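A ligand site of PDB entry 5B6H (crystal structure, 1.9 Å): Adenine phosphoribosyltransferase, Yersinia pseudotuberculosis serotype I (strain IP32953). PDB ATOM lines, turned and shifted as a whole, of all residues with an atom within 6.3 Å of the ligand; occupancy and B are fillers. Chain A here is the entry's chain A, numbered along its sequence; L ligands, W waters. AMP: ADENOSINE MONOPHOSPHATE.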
ATOM      1  N   TYR A  19      20.141  17.833  -2.829  1.00  0.00           N
ATOM      2  CA  TYR A  19      21.561  17.914  -2.605  1.00  0.00           C
ATOM      3  C   TYR A  19      22.074  19.110  -3.392  1.00  0.00           C
ATOM      4  O   TYR A  19      21.570  19.337  -4.470  1.00  0.00           O
ATOM      5  CB  TYR A  19      22.206  16.625  -3.061  1.00  0.00           C
ATOM      6  CG  TYR A  19      23.692  16.657  -2.977  1.00  0.00           C
ATOM      7  CD1 TYR A  19      24.425  17.268  -3.944  1.00  0.00           C
ATOM      8  CD2 TYR A  19      24.365  16.127  -1.874  1.00  0.00           C
ATOM      9  CE1 TYR A  19      25.804  17.346  -3.850  1.00  0.00           C
ATOM     10  CE2 TYR A  19      25.742  16.190  -1.763  1.00  0.00           C
ATOM     11  CZ  TYR A  19      26.463  16.772  -2.750  1.00  0.00           C
ATOM     12  OH  TYR A  19      27.830  16.829  -2.659  1.00  0.00           O
ATOM     13  N   ILE A  24      17.246  22.183  -3.902  1.00  0.00           N
ATOM     14  CA  ILE A  24      18.071  21.987  -5.077  1.00  0.00           C
ATOM     15  C   ILE A  24      17.837  20.586  -5.739  1.00  0.00           C
ATOM     16  O   ILE A  24      17.690  19.562  -5.047  1.00  0.00           O
ATOM     17  CB  ILE A  24      19.559  22.265  -4.750  1.00  0.00           C
ATOM     18  CG1 ILE A  24      19.684  23.637  -4.047  1.00  0.00           C
ATOM     19  CG2 ILE A  24      20.396  22.191  -5.999  1.00  0.00           C
ATOM     20  CD1 ILE A  24      21.069  24.255  -3.997  1.00  0.00           C
ATOM     21  N   LEU A  25      17.738  20.571  -7.072  1.00  0.00           N
ATOM     22  CA  LEU A  25      17.741  19.358  -7.840  1.00  0.00           C
ATOM     23  C   LEU A  25      19.156  19.326  -8.437  1.00  0.00           C
ATOM     24  O   LEU A  25      19.504  20.139  -9.316  1.00  0.00           O
ATOM     25  CB  LEU A  25      16.689  19.345  -8.929  1.00  0.00           C
ATOM     26  CG  LEU A  25      15.223  19.441  -8.567  1.00  0.00           C
ATOM     27  CD1 LEU A  25      14.373  19.887  -9.759  1.00  0.00           C
ATOM     28  CD2 LEU A  25      14.708  18.117  -8.085  1.00  0.00           C
ATOM     29  N   PHE A  26      19.990  18.414  -7.917  1.00  0.00           N
ATOM     30  CA  PHE A  26      21.393  18.391  -8.366  1.00  0.00           C
ATOM     31  C   PHE A  26      21.429  17.548  -9.627  1.00  0.00           C
ATOM     32  O   PHE A  26      20.904  16.441  -9.628  1.00  0.00           O
ATOM     33  CB  PHE A  26      22.304  17.799  -7.285  1.00  0.00           C
ATOM     34  CG  PHE A  26      23.749  17.968  -7.575  1.00  0.00           C
ATOM     35  CD1 PHE A  26      24.374  19.174  -7.298  1.00  0.00           C
ATOM     36  CD2 PHE A  26      24.471  16.987  -8.203  1.00  0.00           C
ATOM     37  CE1 PHE A  26      25.728  19.361  -7.555  1.00  0.00           C
ATOM     38  CE2 PHE A  26      25.857  17.172  -8.480  1.00  0.00           C
ATOM     39  CZ  PHE A  26      26.461  18.352  -8.116  1.00  0.00           C
ATOM     40  N   ARG A  27      22.023  18.043 -10.689  1.00  0.00           N
ATOM     41  CA  ARG A  27      22.198  17.300 -11.890  1.00  0.00           C
ATOM     42  C   ARG A  27      23.614  16.688 -11.883  1.00  0.00           C
ATOM     43  O   ARG A  27      24.610  17.419 -11.958  1.00  0.00           O
ATOM     44  CB  ARG A  27      22.024  18.215 -13.132  1.00  0.00           C
ATOM     45  CG  ARG A  27      20.803  19.126 -13.054  1.00  0.00           C
ATOM     46  CD  ARG A  27      19.503  18.334 -12.961  1.00  0.00           C
ATOM     47  NE  ARG A  27      18.422  19.280 -12.797  1.00  0.00           N
ATOM     48  CZ  ARG A  27      17.116  19.011 -12.872  1.00  0.00           C
ATOM     49  NH1 ARG A  27      16.254  20.002 -12.721  1.00  0.00           N
ATOM     50  NH2 ARG A  27      16.691  17.796 -13.141  1.00  0.00           N
ATOM     51  N   ASP A  28      23.672  15.373 -11.801  1.00  0.00           N
ATOM     52  CA  ASP A  28      24.942  14.646 -11.575  1.00  0.00           C
ATOM     53  C   ASP A  28      25.468  14.186 -12.875  1.00  0.00           C
ATOM     54  O   ASP A  28      24.939  13.152 -13.408  1.00  0.00           O
ATOM     55  CB  ASP A  28      24.707  13.439 -10.623  1.00  0.00           C
ATOM     56  CG  ASP A  28      25.921  12.626 -10.363  1.00  0.00           C
ATOM     57  OD1 ASP A  28      27.067  13.026 -10.695  1.00  0.00           O
ATOM     58  OD2 ASP A  28      25.748  11.496  -9.779  1.00  0.00           O
ATOM     59  N   THR A  61      37.143  25.489 -16.153  1.00  0.00           N
ATOM     60  CA  THR A  61      37.365  25.818 -14.809  1.00  0.00           C
ATOM     61  C   THR A  61      37.388  24.487 -13.993  1.00  0.00           C
ATOM     62  O   THR A  61      36.764  23.471 -14.340  1.00  0.00           O
ATOM     63  CB  THR A  61      36.241  26.669 -14.181  1.00  0.00           C
ATOM     64  OG1 THR A  61      35.055  25.805 -14.239  1.00  0.00           O
ATOM     65  CG2 THR A  61      36.065  28.013 -14.974  1.00  0.00           C
ATOM     66  N   ARG A  64      35.129  20.058 -12.362  1.00  0.00           N
ATOM     67  CA  ARG A  64      34.287  19.285 -13.318  1.00  0.00           C
ATOM     68  C   ARG A  64      34.370  19.857 -14.668  1.00  0.00           C
ATOM     69  O   ARG A  64      34.261  19.104 -15.644  1.00  0.00           O
ATOM     70  CB  ARG A  64      32.836  19.247 -12.877  1.00  0.00           C
ATOM     71  CG  ARG A  64      32.723  18.350 -11.684  1.00  0.00           C
ATOM     72  CD  ARG A  64      31.274  17.905 -11.428  1.00  0.00           C
ATOM     73  NE  ARG A  64      30.549  19.067 -10.943  1.00  0.00           N
ATOM     74  CZ  ARG A  64      30.182  19.325  -9.694  1.00  0.00           C
ATOM     75  NH1 ARG A  64      30.415  18.486  -8.668  1.00  0.00           N
ATOM     76  NH2 ARG A  64      29.568  20.493  -9.436  1.00  0.00           N
ATOM     77  N   TYR A  98      34.393  37.009  -7.801  1.00  0.00           N
ATOM     78  CA  TYR A  98      33.051  36.907  -8.253  1.00  0.00           C
ATOM     79  C   TYR A  98      32.197  36.752  -6.930  1.00  0.00           C
ATOM     80  O   TYR A  98      32.659  36.121  -5.996  1.00  0.00           O
ATOM     81  CB  TYR A  98      32.824  35.773  -9.267  1.00  0.00           C
ATOM     82  CG  TYR A  98      33.211  34.386  -8.884  1.00  0.00           C
ATOM     83  CD1 TYR A  98      34.523  33.896  -9.018  1.00  0.00           C
ATOM     84  CD2 TYR A  98      32.238  33.515  -8.477  1.00  0.00           C
ATOM     85  CE1 TYR A  98      34.826  32.551  -8.645  1.00  0.00           C
ATOM     86  CE2 TYR A  98      32.516  32.231  -8.076  1.00  0.00           C
ATOM     87  CZ  TYR A  98      33.826  31.747  -8.170  1.00  0.00           C
ATOM     88  OH  TYR A  98      34.010  30.472  -7.731  1.00  0.00           O
ATOM     89  N   ASP A 124      32.403  24.168 -19.979  1.00  0.00           N
ATOM     90  CA  ASP A 124      32.150  23.790 -18.576  1.00  0.00           C
ATOM     91  C   ASP A 124      31.101  22.698 -18.468  1.00  0.00           C
ATOM     92  O   ASP A 124      30.390  22.433 -19.442  1.00  0.00           O
ATOM     93  CB  ASP A 124      31.654  25.019 -17.840  1.00  0.00           C
ATOM     94  CG  ASP A 124      31.925  24.994 -16.323  1.00  0.00           C
ATOM     95  OD1 ASP A 124      32.986  24.547 -15.700  1.00  0.00           O
ATOM     96  OD2 ASP A 124      30.990  25.466 -15.659  1.00  0.00           O
ATOM     97  N   ASP A 125      30.838  22.195 -17.263  1.00  0.00           N
ATOM     98  CA  ASP A 125      29.888  21.120 -17.203  1.00  0.00           C
ATOM     99  C   ASP A 125      28.481  21.714 -17.224  1.00  0.00           C
ATOM    100  O   ASP A 125      27.597  21.141 -17.854  1.00  0.00           O
ATOM    101  CB  ASP A 125      30.044  20.254 -15.907  1.00  0.00           C
ATOM    102  CG  ASP A 125      30.109  21.121 -14.599  1.00  0.00           C
ATOM    103  OD1 ASP A 125      30.748  22.150 -14.529  1.00  0.00           O
ATOM    104  OD2 ASP A 125      29.479  20.824 -13.524  1.00  0.00           O
ATOM    105  N   LEU A 126      28.278  22.783 -16.489  1.00  0.00           N
ATOM    106  CA  LEU A 126      26.942  23.257 -16.218  1.00  0.00           C
ATOM    107  C   LEU A 126      26.857  24.782 -16.020  1.00  0.00           C
ATOM    108  O   LEU A 126      27.664  25.364 -15.299  1.00  0.00           O
ATOM    109  CB  LEU A 126      26.307  22.550 -15.023  1.00  0.00           C
ATOM    110  CG  LEU A 126      24.859  22.876 -14.627  1.00  0.00           C
ATOM    111  CD1 LEU A 126      24.233  21.676 -13.951  1.00  0.00           C
ATOM    112  CD2 LEU A 126      24.766  24.081 -13.653  1.00  0.00           C
ATOM    113  N   LEU A 127      25.815  25.383 -16.610  1.00  0.00           N
ATOM    114  CA  LEU A 127      25.563  26.846 -16.445  1.00  0.00           C
ATOM    115  C   LEU A 127      24.427  27.087 -15.472  1.00  0.00           C
ATOM    116  O   LEU A 127      23.294  26.640 -15.717  1.00  0.00           O
ATOM    117  CB  LEU A 127      25.278  27.547 -17.795  1.00  0.00           C
ATOM    118  CG  LEU A 127      24.907  28.980 -17.827  1.00  0.00           C
ATOM    119  CD1 LEU A 127      26.087  29.768 -17.247  1.00  0.00           C
ATOM    120  CD2 LEU A 127      24.576  29.347 -19.286  1.00  0.00           C
ATOM    121  N   ALA A 128      24.765  27.747 -14.362  1.00  0.00           N
ATOM    122  CA  ALA A 128      23.712  28.024 -13.347  1.00  0.00           C
ATOM    123  C   ALA A 128      23.524  29.522 -13.282  1.00  0.00           C
ATOM    124  O   ALA A 128      22.816  30.087 -14.162  1.00  0.00           O
ATOM    125  CB  ALA A 128      24.076  27.368 -12.015  1.00  0.00           C
ATOM    126  N   THR A 129      24.235  30.189 -12.371  1.00  0.00           N
ATOM    127  CA  THR A 129      24.148  31.651 -12.245  1.00  0.00           C
ATOM    128  C   THR A 129      25.024  32.343 -13.220  1.00  0.00           C
ATOM    129  O   THR A 129      24.754  33.500 -13.556  1.00  0.00           O
ATOM    130  CB  THR A 129      24.594  32.145 -10.888  1.00  0.00           C
ATOM    131  OG1 THR A 129      25.977  31.878 -10.669  1.00  0.00           O
ATOM    132  CG2 THR A 129      23.781  31.497  -9.755  1.00  0.00           C
ATOM    133  N   GLY A 130      26.041  31.669 -13.730  1.00  0.00           N
ATOM    134  CA  GLY A 130      26.972  32.303 -14.614  1.00  0.00           C
ATOM    135  C   GLY A 130      28.104  33.030 -13.912  1.00  0.00           C
ATOM    136  O   GLY A 130      28.998  33.546 -14.540  1.00  0.00           O
ATOM    137  N   GLY A 131      28.164  33.047 -12.591  1.00  0.00           N
ATOM    138  CA  GLY A 131      29.200  33.828 -11.980  1.00  0.00           C
ATOM    139  C   GLY A 131      30.607  33.325 -12.291  1.00  0.00           C
ATOM    140  O   GLY A 131      31.530  34.126 -12.463  1.00  0.00           O
ATOM    141  N   THR A 132      30.837  31.961 -12.281  1.00  0.00           N
ATOM    142  CA  THR A 132      32.181  31.532 -12.571  1.00  0.00           C
ATOM    143  C   THR A 132      32.618  31.850 -13.965  1.00  0.00           C
ATOM    144  O   THR A 132      33.746  32.109 -14.194  1.00  0.00           O
ATOM    145  CB  THR A 132      32.392  30.028 -12.328  1.00  0.00           C
ATOM    146  OG1 THR A 132      31.263  29.348 -12.865  1.00  0.00           O
ATOM    147  CG2 THR A 132      32.241  29.772 -10.854  1.00  0.00           C
ATOM    148  N   ILE A 133      31.725  31.675 -14.927  1.00  0.00           N
ATOM    149  CA  ILE A 133      32.035  31.886 -16.312  1.00  0.00           C
ATOM    150  C   ILE A 133      32.257  33.394 -16.631  1.00  0.00           C
ATOM    151  O   ILE A 133      33.135  33.770 -17.417  1.00  0.00           O
ATOM    152  CB  ILE A 133      30.910  31.360 -17.240  1.00  0.00           C
ATOM    153  CG1 ILE A 133      30.673  29.877 -17.052  1.00  0.00           C
ATOM    154  CG2 ILE A 133      31.411  31.527 -18.677  1.00  0.00           C
ATOM    155  CD1 ILE A 133      31.954  29.099 -17.152  1.00  0.00           C
ATOM    156  N   PHE A 152      28.451  24.202 -22.716  1.00  0.00           N
ATOM    157  CA  PHE A 152      28.184  23.450 -21.503  1.00  0.00           C
ATOM    158  C   PHE A 152      27.528  22.139 -21.834  1.00  0.00           C
ATOM    159  O   PHE A 152      26.799  22.011 -22.855  1.00  0.00           O
ATOM    160  CB  PHE A 152      27.222  24.224 -20.653  1.00  0.00           C
ATOM    161  CG  PHE A 152      27.695  25.605 -20.334  1.00  0.00           C
ATOM    162  CD1 PHE A 152      28.454  25.850 -19.232  1.00  0.00           C
ATOM    163  CD2 PHE A 152      27.433  26.696 -21.218  1.00  0.00           C
ATOM    164  CE1 PHE A 152      28.886  27.147 -18.922  1.00  0.00           C
ATOM    165  CE2 PHE A 152      27.857  27.918 -20.932  1.00  0.00           C
ATOM    166  CZ  PHE A 152      28.572  28.166 -19.788  1.00  0.00           C
ATOM    167  N   LEU A 156      20.883  25.583 -16.892  1.00  0.00           N
ATOM    168  CA  LEU A 156      19.704  25.737 -16.013  1.00  0.00           C
ATOM    169  C   LEU A 156      19.174  27.161 -16.209  1.00  0.00           C
ATOM    170  O   LEU A 156      19.564  28.080 -15.534  1.00  0.00           O
ATOM    171  CB  LEU A 156      20.023  25.451 -14.524  1.00  0.00           C
ATOM    172  CG  LEU A 156      20.733  24.141 -14.240  1.00  0.00           C
ATOM    173  CD1 LEU A 156      21.163  24.047 -12.797  1.00  0.00           C
ATOM    174  CD2 LEU A 156      19.815  22.961 -14.603  1.00  0.00           C
ATOM    175  N   LEU A 159      18.056  29.864 -13.575  1.00  0.00           N
ATOM    176  CA  LEU A 159      18.976  30.549 -12.720  1.00  0.00           C
ATOM    177  C   LEU A 159      19.650  31.766 -13.337  1.00  0.00           C
ATOM    178  O   LEU A 159      20.416  32.402 -12.661  1.00  0.00           O
ATOM    179  CB  LEU A 159      20.035  29.604 -12.157  1.00  0.00           C
ATOM    180  CG  LEU A 159      19.452  28.465 -11.289  1.00  0.00           C
ATOM    181  CD1 LEU A 159      20.526  27.440 -11.018  1.00  0.00           C
ATOM    182  CD2 LEU A 159      18.912  28.980  -9.969  1.00  0.00           C
ATOM    183  N   GLY A 161      21.970  32.452 -15.909  1.00  0.00           N
ATOM    184  CA  GLY A 161      23.353  32.618 -16.309  1.00  0.00           C
ATOM    185  C   GLY A 161      23.526  32.961 -17.775  1.00  0.00           C
ATOM    186  O   GLY A 161      24.404  33.726 -18.184  1.00  0.00           O
HETATM  187  P   AMP L   1      27.591  29.135 -11.838  1.00  0.00           P
HETATM  188  O1P AMP L   1      26.519  29.476 -10.731  1.00  0.00           O
HETATM  189  O2P AMP L   1      27.052  29.034 -13.266  1.00  0.00           O
HETATM  190  O3P AMP L   1      28.889  29.823 -11.603  1.00  0.00           O
HETATM  191  O5' AMP L   1      27.929  27.475 -11.547  1.00  0.00           O
HETATM  192  C5' AMP L   1      29.097  27.025 -10.887  1.00  0.00           C
HETATM  193  C4' AMP L   1      29.002  25.436 -10.867  1.00  0.00           C
HETATM  194  O4' AMP L   1      28.025  25.075  -9.850  1.00  0.00           O
HETATM  195  C3' AMP L   1      28.525  24.816 -12.172  1.00  0.00           C
HETATM  196  O3' AMP L   1      29.556  24.823 -13.199  1.00  0.00           O
HETATM  197  C2' AMP L   1      28.072  23.462 -11.631  1.00  0.00           C
HETATM  198  O2' AMP L   1      29.284  22.671 -11.532  1.00  0.00           O
HETATM  199  C1' AMP L   1      27.534  23.746 -10.235  1.00  0.00           C
HETATM  200  N9  AMP L   1      26.064  23.668 -10.103  1.00  0.00           N
HETATM  201  C8  AMP L   1      25.232  24.680  -9.785  1.00  0.00           C
HETATM  202  N7  AMP L   1      23.948  24.246  -9.671  1.00  0.00           N
HETATM  203  C5  AMP L   1      23.963  22.984  -9.949  1.00  0.00           C
HETATM  204  C6  AMP L   1      22.981  21.928  -9.964  1.00  0.00           C
HETATM  205  N6  AMP L   1      21.688  22.165  -9.743  1.00  0.00           N
HETATM  206  N1  AMP L   1      23.414  20.692 -10.220  1.00  0.00           N
HETATM  207  C2  AMP L   1      24.710  20.396 -10.448  1.00  0.00           C
HETATM  208  N3  AMP L   1      25.670  21.300 -10.413  1.00  0.00           N
HETATM  209  C4  AMP L   1      25.339  22.589 -10.198  1.00  0.00           C
HETATM  210  O   HOH W   1      29.131  30.661  -8.985  1.00  0.00           O
HETATM  211  O   HOH W   2      29.150  27.552 -15.130  1.00  0.00           O
HETATM  212  O   HOH W   3      27.593  19.724 -12.285  1.00  0.00           O
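An oxygen (O1P) of the ligand is in hydrogen-bond range of the backbone NH of Thr 129 (2.9 Å). The side-chain hydroxyl (OG1) of Thr 129 lies within hydrogen-bond range of an oxygen (O1P) of the ligand (2.5 Å). The side-chain carboxylate (OD2) of Asp 125 lies within hydrogen-bond range of an oxygen (O2') of the ligand, 2.7 Å away. An oxygen (O3P) of the ligand is in hydrogen-bond range of the backbone NH of Thr 132 (3.0 Å). An oxygen (O3P) of the ligand is in hydrogen-bond range of the side-chain hydroxyl (OG1) of Thr 132. O2P of the ligand sits at hydrogen-bond distance from N of Ala 128, at 2.8 Å. N of Gly 130 is in hydrogen-bond range of O2P of the ligand (2.9 Å). The backbone carbonyl oxygen (O) of Leu 126 is in hydrogen-bond range of an oxygen (O3') of the ligand. The side-chain carboxylate of Asp 124 sits at hydrogen-bond distance from an oxygen (O3') of the ligand. The backbone carbonyl oxygen (O) of Leu 25 lies within hydrogen-bond range of a nitrogen (N6) of the ligand (3.0 Å). A nitrogen (N1) of the ligand sits at hydrogen-bond distance from the backbone NH of Arg 27, 3.0 Å away. NH2 of Arg 64 is in hydrogen-bond range of O2' of the ligand (3.0 Å). The backbone NH of Gly 131 sits at hydrogen-bond distance from an oxygen (O3P) of the ligand.
N of Gly 131 sits at hydrogen-bond distance from OG1 of Thr 129, 3.1 Å away. The side-chain carboxylate of Asp 125 lies within salt-bridge range of the guanidinium group of Arg 64 (3.3 Å). O of Ala 128 is in hydrogen-bond range of N of Gly 161 (3.1 Å). OD1 of Asp 124 sits at hydrogen-bond distance from OG1 of Thr 61. N of Leu 156 lies within hydrogen-bond range of O of Leu 127, at 2.9 Å.
Merely in contact with the ligand: Phe 26 (3.2 Å), Leu 156 (3.6 Å), Leu 127 (3.9 Å) and Ile 24 (3.96 Å). Hydrophobic or aromatic side chains that line the ligand: Ile 24, Phe 26, Leu 126, Ala 128 and Leu 156. 15 residues have an atom within 4 Å of the ligand: Ile 24, Leu 25, Phe 26, Arg 27, Arg 64, Asp 124, Asp 125, Leu 126, Leu 127, Ala 128, Thr 129, Gly 130, Gly 131, Thr 132 and Leu 156.
Water W3 lies within hydrogen-bond range of OD2 of Asp 125 (2.5 Å), N3 of the ligand (3.1 Å) and NE of Arg 64 (3.3 Å). Water W2 lies within hydrogen-bond range of O of Leu 126 (2.7 Å), OD2 of Asp 124 (2.8 Å) and O2P of the ligand (3.2 Å).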
